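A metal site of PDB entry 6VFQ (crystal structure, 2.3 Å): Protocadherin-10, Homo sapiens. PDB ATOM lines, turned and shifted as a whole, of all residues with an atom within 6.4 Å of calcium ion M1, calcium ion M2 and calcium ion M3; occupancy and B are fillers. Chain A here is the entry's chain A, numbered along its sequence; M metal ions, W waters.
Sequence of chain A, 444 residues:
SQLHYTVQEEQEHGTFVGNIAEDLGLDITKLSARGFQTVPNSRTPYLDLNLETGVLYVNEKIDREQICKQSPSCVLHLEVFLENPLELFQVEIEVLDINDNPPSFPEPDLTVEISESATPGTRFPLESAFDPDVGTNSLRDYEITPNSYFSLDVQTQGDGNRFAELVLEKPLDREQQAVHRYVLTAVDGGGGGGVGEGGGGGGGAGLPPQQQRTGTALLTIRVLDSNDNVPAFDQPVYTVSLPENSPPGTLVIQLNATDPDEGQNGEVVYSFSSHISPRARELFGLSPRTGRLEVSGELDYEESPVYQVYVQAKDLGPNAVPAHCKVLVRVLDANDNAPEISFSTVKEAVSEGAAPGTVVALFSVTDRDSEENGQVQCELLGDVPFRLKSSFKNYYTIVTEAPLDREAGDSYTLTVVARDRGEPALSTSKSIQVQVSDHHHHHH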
ATOM      1  N   GLU A 244       6.667  -1.994   6.811  1.00  0.00           N
ATOM      2  CA  GLU A 244       7.175  -3.065   7.645  1.00  0.00           C
ATOM      3  C   GLU A 244       8.208  -3.857   6.871  1.00  0.00           C
ATOM      4  O   GLU A 244       8.247  -3.846   5.634  1.00  0.00           O
ATOM      5  CB  GLU A 244       6.034  -3.973   8.133  1.00  0.00           C
ATOM      6  CG  GLU A 244       5.502  -4.926   7.093  1.00  0.00           C
ATOM      7  CD  GLU A 244       4.467  -5.936   7.613  1.00  0.00           C
ATOM      8  OE1 GLU A 244       4.665  -6.535   8.703  1.00  0.00           O
ATOM      9  OE2 GLU A 244       3.466  -6.141   6.898  1.00  0.00           O
ATOM     10  N   ASN A 245       9.069  -4.534   7.595  1.00  0.00           N
ATOM     11  CA  ASN A 245      10.201  -5.243   6.996  1.00  0.00           C
ATOM     12  C   ASN A 245      11.200  -4.302   6.300  1.00  0.00           C
ATOM     13  O   ASN A 245      12.055  -4.770   5.532  1.00  0.00           O
ATOM     14  CB  ASN A 245       9.704  -6.318   6.014  1.00  0.00           C
ATOM     15  CG  ASN A 245       8.691  -7.257   6.646  1.00  0.00           C
ATOM     16  OD1 ASN A 245       8.847  -7.661   7.806  1.00  0.00           O
ATOM     17  ND2 ASN A 245       7.652  -7.603   5.904  1.00  0.00           N
ATOM     18  N   LEU A 299      10.836  -4.146  11.624  1.00  0.00           N
ATOM     19  CA  LEU A 299       9.547  -3.542  11.882  1.00  0.00           C
ATOM     20  C   LEU A 299       8.456  -4.497  11.432  1.00  0.00           C
ATOM     21  O   LEU A 299       8.347  -4.787  10.228  1.00  0.00           O
ATOM     22  CB  LEU A 299       9.429  -2.228  11.141  1.00  0.00           C
ATOM     23  CG  LEU A 299      10.471  -1.194  11.556  1.00  0.00           C
ATOM     24  CD1 LEU A 299      10.386   0.053  10.682  1.00  0.00           C
ATOM     25  CD2 LEU A 299      10.278  -0.820  13.016  1.00  0.00           C
ATOM     26  N   ASP A 300       7.655  -4.985  12.370  1.00  0.00           N
ATOM     27  CA  ASP A 300       6.574  -5.928  12.085  1.00  0.00           C
ATOM     28  C   ASP A 300       5.229  -5.257  12.372  1.00  0.00           C
ATOM     29  O   ASP A 300       4.884  -5.030  13.535  1.00  0.00           O
ATOM     30  CB  ASP A 300       6.728  -7.210  12.896  1.00  0.00           C
ATOM     31  CG  ASP A 300       5.563  -8.162  12.697  1.00  0.00           C
ATOM     32  OD1 ASP A 300       4.739  -7.958  11.765  1.00  0.00           O
ATOM     33  OD2 ASP A 300       5.465  -9.128  13.469  1.00  0.00           O
ATOM     34  N   TYR A 301       4.469  -4.966  11.319  1.00  0.00           N
ATOM     35  CA  TYR A 301       3.141  -4.378  11.479  1.00  0.00           C
ATOM     36  C   TYR A 301       2.256  -5.248  12.375  1.00  0.00           C
ATOM     37  O   TYR A 301       1.546  -4.737  13.248  1.00  0.00           O
ATOM     38  CB  TYR A 301       2.486  -4.205  10.115  1.00  0.00           C
ATOM     39  CG  TYR A 301       1.128  -3.584  10.176  1.00  0.00           C
ATOM     40  CD1 TYR A 301      -0.014  -4.355  10.333  1.00  0.00           C
ATOM     41  CD2 TYR A 301       0.986  -2.218  10.080  1.00  0.00           C
ATOM     42  CE1 TYR A 301      -1.285  -3.757  10.392  1.00  0.00           C
ATOM     43  CE2 TYR A 301      -0.248  -1.622  10.134  1.00  0.00           C
ATOM     44  CZ  TYR A 301      -1.377  -2.380  10.298  1.00  0.00           C
ATOM     45  OH  TYR A 301      -2.588  -1.731  10.347  1.00  0.00           O
ATOM     46  N   GLU A 302       2.277  -6.568  12.167  1.00  0.00           N
ATOM     47  CA  GLU A 302       1.426  -7.431  12.953  1.00  0.00           C
ATOM     48  C   GLU A 302       1.829  -7.461  14.420  1.00  0.00           C
ATOM     49  O   GLU A 302       1.097  -8.038  15.230  1.00  0.00           O
ATOM     50  CB  GLU A 302       1.415  -8.853  12.367  1.00  0.00           C
ATOM     51  CG  GLU A 302       0.617  -8.973  11.068  1.00  0.00           C
ATOM     52  CD  GLU A 302       1.316  -8.388   9.836  1.00  0.00           C
ATOM     53  OE1 GLU A 302       2.505  -8.710   9.582  1.00  0.00           O
ATOM     54  OE2 GLU A 302       0.664  -7.609   9.098  1.00  0.00           O
ATOM     55  N   GLU A 303       2.961  -6.864  14.778  1.00  0.00           N
ATOM     56  CA  GLU A 303       3.354  -6.686  16.168  1.00  0.00           C
ATOM     57  C   GLU A 303       2.908  -5.341  16.718  1.00  0.00           C
ATOM     58  O   GLU A 303       2.389  -5.263  17.835  1.00  0.00           O
ATOM     59  CB  GLU A 303       4.868  -6.820  16.300  1.00  0.00           C
ATOM     60  CG  GLU A 303       5.390  -6.689  17.717  1.00  0.00           C
ATOM     61  CD  GLU A 303       6.903  -6.708  17.769  1.00  0.00           C
ATOM     62  OE1 GLU A 303       7.536  -6.737  16.688  1.00  0.00           O
ATOM     63  OE2 GLU A 303       7.466  -6.689  18.894  1.00  0.00           O
ATOM     64  N   LEU A 332       3.704   0.511   8.004  1.00  0.00           N
ATOM     65  CA  LEU A 332       2.758   0.226   6.934  1.00  0.00           C
ATOM     66  C   LEU A 332       2.727  -1.272   6.686  1.00  0.00           C
ATOM     67  O   LEU A 332       3.779  -1.914   6.599  1.00  0.00           O
ATOM     68  CB  LEU A 332       3.141   0.970   5.660  1.00  0.00           C
ATOM     69  CG  LEU A 332       3.220   2.479   5.797  1.00  0.00           C
ATOM     70  CD1 LEU A 332       3.709   3.066   4.489  1.00  0.00           C
ATOM     71  CD2 LEU A 332       1.864   3.052   6.156  1.00  0.00           C
ATOM     72  N   ASP A 333       1.525  -1.827   6.610  1.00  0.00           N
ATOM     73  CA  ASP A 333       1.358  -3.264   6.465  1.00  0.00           C
ATOM     74  C   ASP A 333       1.773  -3.701   5.063  1.00  0.00           C
ATOM     75  O   ASP A 333       1.410  -3.070   4.075  1.00  0.00           O
ATOM     76  CB  ASP A 333      -0.102  -3.631   6.764  1.00  0.00           C
ATOM     77  CG  ASP A 333      -0.463  -5.089   6.413  1.00  0.00           C
ATOM     78  OD1 ASP A 333       0.136  -6.068   6.948  1.00  0.00           O
ATOM     79  OD2 ASP A 333      -1.405  -5.230   5.603  1.00  0.00           O
ATOM     80  N   ALA A 334       2.565  -4.769   5.001  1.00  0.00           N
ATOM     81  CA  ALA A 334       2.873  -5.485   3.777  1.00  0.00           C
ATOM     82  C   ALA A 334       2.175  -6.857   3.770  1.00  0.00           C
ATOM     83  O   ALA A 334       1.651  -7.319   4.779  1.00  0.00           O
ATOM     84  CB  ALA A 334       4.389  -5.676   3.640  1.00  0.00           C
ATOM     85  N   ASN A 335       2.219  -7.534   2.613  1.00  0.00           N
ATOM     86  CA  ASN A 335       1.612  -8.861   2.492  1.00  0.00           C
ATOM     87  C   ASN A 335       2.682  -9.906   2.742  1.00  0.00           C
ATOM     88  O   ASN A 335       3.238 -10.517   1.832  1.00  0.00           O
ATOM     89  CB  ASN A 335       0.944  -9.045   1.134  1.00  0.00           C
ATOM     90  CG  ASN A 335       0.057 -10.320   1.086  1.00  0.00           C
ATOM     91  OD1 ASN A 335      -0.404 -10.818   2.106  1.00  0.00           O
ATOM     92  ND2 ASN A 335      -0.156 -10.847  -0.119  1.00  0.00           N
ATOM     93  N   ASP A 336       2.947 -10.139   4.025  1.00  0.00           N
ATOM     94  CA  ASP A 336       3.945 -11.114   4.443  1.00  0.00           C
ATOM     95  C   ASP A 336       3.356 -12.288   5.213  1.00  0.00           C
ATOM     96  O   ASP A 336       4.124 -13.059   5.805  1.00  0.00           O
ATOM     97  CB  ASP A 336       5.040 -10.421   5.264  1.00  0.00           C
ATOM     98  CG  ASP A 336       4.507  -9.585   6.442  1.00  0.00           C
ATOM     99  OD1 ASP A 336       3.279  -9.315   6.522  1.00  0.00           O
ATOM    100  OD2 ASP A 336       5.344  -9.204   7.291  1.00  0.00           O
ATOM    101  N   ASN A 337       2.043 -12.475   5.225  1.00  0.00           N
ATOM    102  CA  ASN A 337       1.454 -13.695   5.766  1.00  0.00           C
ATOM    103  C   ASN A 337       0.558 -14.363   4.723  1.00  0.00           C
ATOM    104  O   ASN A 337      -0.284 -13.710   4.097  1.00  0.00           O
ATOM    105  CB  ASN A 337       0.663 -13.410   7.039  1.00  0.00           C
ATOM    106  CG  ASN A 337       1.560 -12.966   8.176  1.00  0.00           C
ATOM    107  OD1 ASN A 337       2.109 -13.779   8.914  1.00  0.00           O
ATOM    108  ND2 ASN A 337       1.712 -11.666   8.332  1.00  0.00           N
ATOM    109  N   ALA A 338       0.726 -15.599   4.569  1.00  0.00           N
ATOM    110  CA  ALA A 338      -0.124 -16.332   3.659  1.00  0.00           C
ATOM    111  C   ALA A 338      -1.383 -16.818   4.374  1.00  0.00           C
ATOM    112  O   ALA A 338      -1.359 -17.039   5.590  1.00  0.00           O
ATOM    113  CB  ALA A 338       0.625 -17.522   3.075  1.00  0.00           C
ATOM    114  N   PRO A 339      -2.481 -16.981   3.641  1.00  0.00           N
ATOM    115  CA  PRO A 339      -3.708 -17.543   4.243  1.00  0.00           C
ATOM    116  C   PRO A 339      -3.475 -18.874   4.945  1.00  0.00           C
ATOM    117  O   PRO A 339      -2.622 -19.670   4.548  1.00  0.00           O
ATOM    118  CB  PRO A 339      -4.622 -17.725   3.024  1.00  0.00           C
ATOM    119  CG  PRO A 339      -4.148 -16.726   2.031  1.00  0.00           C
ATOM    120  CD  PRO A 339      -2.681 -16.567   2.252  1.00  0.00           C
ATOM    121  N   ASP A 367      -6.014 -14.967   7.624  1.00  0.00           N
ATOM    122  CA  ASP A 367      -4.818 -14.299   7.105  1.00  0.00           C
ATOM    123  C   ASP A 367      -4.409 -13.202   8.089  1.00  0.00           C
ATOM    124  O   ASP A 367      -5.195 -12.285   8.353  1.00  0.00           O
ATOM    125  CB  ASP A 367      -5.103 -13.710   5.701  1.00  0.00           C
ATOM    126  CG  ASP A 367      -3.827 -13.237   4.981  1.00  0.00           C
ATOM    127  OD1 ASP A 367      -3.046 -12.448   5.558  1.00  0.00           O
ATOM    128  OD2 ASP A 367      -3.613 -13.649   3.820  1.00  0.00           O
ATOM    129  N   ARG A 368      -3.200 -13.303   8.644  1.00  0.00           N
ATOM    130  CA  ARG A 368      -2.782 -12.384   9.703  1.00  0.00           C
ATOM    131  C   ARG A 368      -2.636 -10.942   9.234  1.00  0.00           C
ATOM    132  O   ARG A 368      -2.482 -10.045  10.076  1.00  0.00           O
ATOM    133  CB  ARG A 368      -1.445 -12.815  10.327  1.00  0.00           C
ATOM    134  CG  ARG A 368      -1.421 -14.234  10.926  1.00  0.00           C
ATOM    135  CD  ARG A 368      -0.693 -14.323  12.278  1.00  0.00           C
ATOM    136  NE  ARG A 368       0.636 -13.717  12.244  1.00  0.00           N
ATOM    137  CZ  ARG A 368       1.062 -12.729  13.035  1.00  0.00           C
ATOM    138  NH1 ARG A 368       0.265 -12.209  13.967  1.00  0.00           N
ATOM    139  NH2 ARG A 368       2.300 -12.263  12.897  1.00  0.00           N
ATOM    140  N   ASP A 369      -2.677 -10.704   7.927  1.00  0.00           N
ATOM    141  CA  ASP A 369      -2.519  -9.368   7.384  1.00  0.00           C
ATOM    142  C   ASP A 369      -3.844  -8.598   7.496  1.00  0.00           C
ATOM    143  O   ASP A 369      -4.845  -9.097   8.011  1.00  0.00           O
ATOM    144  CB  ASP A 369      -2.017  -9.445   5.946  1.00  0.00           C
ATOM    145  CG  ASP A 369      -0.612 -10.020   5.849  1.00  0.00           C
ATOM    146  OD1 ASP A 369       0.256  -9.610   6.668  1.00  0.00           O
ATOM    147  OD2 ASP A 369      -0.361 -10.890   4.980  1.00  0.00           O
ATOM    148  N   SER A 370      -3.854  -7.369   6.986  1.00  0.00           N
ATOM    149  CA  SER A 370      -4.988  -6.453   7.118  1.00  0.00           C
ATOM    150  C   SER A 370      -5.376  -5.938   5.734  1.00  0.00           C
ATOM    151  O   SER A 370      -4.585  -5.967   4.798  1.00  0.00           O
ATOM    152  CB  SER A 370      -4.651  -5.272   8.039  1.00  0.00           C
ATOM    153  OG  SER A 370      -4.216  -5.707   9.319  1.00  0.00           O
ATOM    154  N   GLU A 372      -6.748  -5.585   2.024  1.00  0.00           N
ATOM    155  CA  GLU A 372      -6.537  -6.502   0.915  1.00  0.00           C
ATOM    156  C   GLU A 372      -5.530  -7.586   1.243  1.00  0.00           C
ATOM    157  O   GLU A 372      -5.661  -8.725   0.783  1.00  0.00           O
ATOM    158  CB  GLU A 372      -6.063  -5.733  -0.319  1.00  0.00           C
ATOM    159  CG  GLU A 372      -7.089  -4.792  -0.941  1.00  0.00           C
ATOM    160  CD  GLU A 372      -6.483  -3.927  -2.031  1.00  0.00           C
ATOM    161  OE1 GLU A 372      -5.233  -3.829  -2.098  1.00  0.00           O
ATOM    162  OE2 GLU A 372      -7.250  -3.342  -2.839  1.00  0.00           O
ATOM    163  N   ASN A 373      -4.474  -7.253   1.979  1.00  0.00           N
ATOM    164  CA  ASN A 373      -3.466  -8.268   2.255  1.00  0.00           C
ATOM    165  C   ASN A 373      -4.036  -9.407   3.092  1.00  0.00           C
ATOM    166  O   ASN A 373      -3.434 -10.490   3.129  1.00  0.00           O
ATOM    167  CB  ASN A 373      -2.256  -7.657   2.963  1.00  0.00           C
ATOM    168  CG  ASN A 373      -1.625  -6.524   2.166  1.00  0.00           C
ATOM    169  OD1 ASN A 373      -1.409  -6.634   0.954  1.00  0.00           O
ATOM    170  ND2 ASN A 373      -1.323  -5.426   2.855  1.00  0.00           N
ATOM    171  N   GLY A 374      -5.161  -9.182   3.771  1.00  0.00           N
ATOM    172  CA  GLY A 374      -5.805 -10.185   4.594  1.00  0.00           C
ATOM    173  C   GLY A 374      -7.120 -10.688   4.045  1.00  0.00           C
ATOM    174  O   GLY A 374      -7.812 -11.436   4.738  1.00  0.00           O
ATOM    175  N   GLN A 375      -7.500 -10.305   2.823  1.00  0.00           N
ATOM    176  CA  GLN A 375      -8.708 -10.767   2.164  1.00  0.00           C
ATOM    177  C   GLN A 375      -8.396 -12.024   1.370  1.00  0.00           C
ATOM    178  O   GLN A 375      -7.464 -12.032   0.562  1.00  0.00           O
ATOM    179  CB  GLN A 375      -9.248  -9.697   1.216  1.00  0.00           C
ATOM    180  CG  GLN A 375     -10.078  -8.636   1.860  1.00  0.00           C
ATOM    181  CD  GLN A 375     -10.482  -7.573   0.845  1.00  0.00           C
ATOM    182  OE1 GLN A 375      -9.941  -7.527  -0.269  1.00  0.00           O
ATOM    183  NE2 GLN A 375     -11.429  -6.722   1.220  1.00  0.00           N
ATOM    184  N   ASP A 420      -4.783 -14.746  -0.941  1.00  0.00           N
ATOM    185  CA  ASP A 420      -5.107 -13.386  -0.534  1.00  0.00           C
ATOM    186  C   ASP A 420      -4.960 -12.443  -1.733  1.00  0.00           C
ATOM    187  O   ASP A 420      -4.510 -12.830  -2.804  1.00  0.00           O
ATOM    188  CB  ASP A 420      -4.245 -12.905   0.654  1.00  0.00           C
ATOM    189  CG  ASP A 420      -2.768 -12.806   0.330  1.00  0.00           C
ATOM    190  OD1 ASP A 420      -2.412 -12.381  -0.782  1.00  0.00           O
ATOM    191  OD2 ASP A 420      -1.950 -13.152   1.206  1.00  0.00           O
ATOM    192  N   ARG A 421      -5.292 -11.176  -1.507  1.00  0.00           N
ATOM    193  CA  ARG A 421      -5.376 -10.164  -2.554  1.00  0.00           C
ATOM    194  C   ARG A 421      -4.331  -9.064  -2.395  1.00  0.00           C
ATOM    195  O   ARG A 421      -4.591  -7.906  -2.730  1.00  0.00           O
ATOM    196  CB  ARG A 421      -6.783  -9.569  -2.581  1.00  0.00           C
ATOM    197  CG  ARG A 421      -7.815 -10.544  -3.161  1.00  0.00           C
ATOM    198  CD  ARG A 421      -9.134  -9.865  -3.407  1.00  0.00           C
ATOM    199  NE  ARG A 421      -9.057  -8.807  -4.413  1.00  0.00           N
ATOM    200  CZ  ARG A 421      -9.146  -9.003  -5.726  1.00  0.00           C
ATOM    201  NH1 ARG A 421      -9.294 -10.223  -6.224  1.00  0.00           N
ATOM    202  NH2 ARG A 421      -9.087  -7.959  -6.551  1.00  0.00           N
ATOM    203  N   GLY A 422      -3.151  -9.420  -1.890  1.00  0.00           N
ATOM    204  CA  GLY A 422      -2.018  -8.514  -1.862  1.00  0.00           C
ATOM    205  C   GLY A 422      -1.196  -8.546  -3.144  1.00  0.00           C
ATOM    206  O   GLY A 422      -1.505  -9.274  -4.091  1.00  0.00           O
ATOM    207  N   LEU A 426      -0.288 -14.161  -2.078  1.00  0.00           N
ATOM    208  CA  LEU A 426       0.172 -15.364  -1.416  1.00  0.00           C
ATOM    209  C   LEU A 426      -0.981 -16.335  -1.337  1.00  0.00           C
ATOM    210  O   LEU A 426      -2.138 -15.940  -1.231  1.00  0.00           O
ATOM    211  CB  LEU A 426       0.697 -15.051  -0.018  1.00  0.00           C
ATOM    212  CG  LEU A 426       1.946 -14.172  -0.067  1.00  0.00           C
ATOM    213  CD1 LEU A 426       2.289 -13.711   1.320  1.00  0.00           C
ATOM    214  CD2 LEU A 426       3.096 -14.945  -0.689  1.00  0.00           C
HETATM  215 CA    CA M   1       4.775  -8.825   9.508  1.00  0.00          CA
HETATM  216 CA    CA M   2       1.764  -7.763   7.123  1.00  0.00          CA
HETATM  217 CA    CA M   3      -1.750 -12.107   3.451  1.00  0.00          CA
HETATM  218  O   HOH W   1       4.502 -11.108  10.204  1.00  0.00           O
HETATM  219  O   HOH W   2       7.288  -8.616   9.910  1.00  0.00           O
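Calcium ion M3 is bound by the backbone carbonyl oxygen (O) of Asn 337, the side-chain amide oxygen (OD1) of Asn 335, the backbone carbonyl oxygen (O) of Asn 373, the side-chain carboxylate (OD2) of Asp 369, the side-chain carboxylate (OD2) of Asp 367, the side-chain carboxylate (OD2) of Asp 420 and the side-chain carboxylate (OD1) of Asp 367. Calcium ion M3 has seven donor atoms within binding distance.
Of the 27 residues printed, 6 come within 4 Å of calcium ion M3. The nearest printed residue that does not touch calcium ion M3 is Ala 338 (4.4 Å).
Calcium ion M1 is bound by OE1 of Glu 302. OD2 of Asp 336 binds calcium ion M1 (2.3 Å). Water W1 binds calcium ion M1, 2.4 Å away. The side-chain carboxylate (OD1) of Asp 300 is bound to calcium ion M1 (2.4 Å). Calcium ion M1 is bound by OE1 of Glu 244, at 2.4 Å. Water W2 is bound to calcium ion M1 (2.6 Å). Calcium ion M1 has six donor atoms within binding distance.
Calcium ion M2 is bound by OD1 of Asp 336, OE2 of Glu 302, OD1 of Asp 333, OE2 of Glu 244, O of Ala 334, OD1 of Asp 369 and OE1 of Glu 302. Calcium ion M2 has seven donor atoms within binding distance.
Of the 27 residues printed, 4 come within 4 Å of calcium ion M1.
The backbone NH (N) of Glu 244 lies within hydrogen-bond range of the backbone carbonyl oxygen (O) of Leu 332 (2.9 Å). OE1 of Glu 302 lies close to ND2 of Asn 337 (3.3 Å). OD1 of Asp 336 lies close to ND2 of Asn 337, at 3.4 Å. The side-chain carboxylate (OE1) of Glu 244 sits close to the backbone NH (N) of Tyr 301 (3.1 Å). The side-chain carboxylate (OD1) of Asp 420 is in hydrogen-bond range of the backbone NH (N) of Gly 422 (3.2 Å). ND2 of Asn 373 sits at hydrogen-bond distance from OD2 of Asp 333. O of Leu 426 sits at hydrogen-bond distance from N of Asp 420 (2.9 Å). The side-chain carboxylate of Asp 336 sits close to the side-chain amide nitrogen of Asn 245, 3.1 Å away.
Six residues have an atom within 4 Å of calcium ion M2: Glu 244, Glu 302, Asp 333, Ala 334, Asp 336 and Asp 369. The nearest printed residue that does not touch calcium ion M2 is Asn 337 (4.1 Å).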
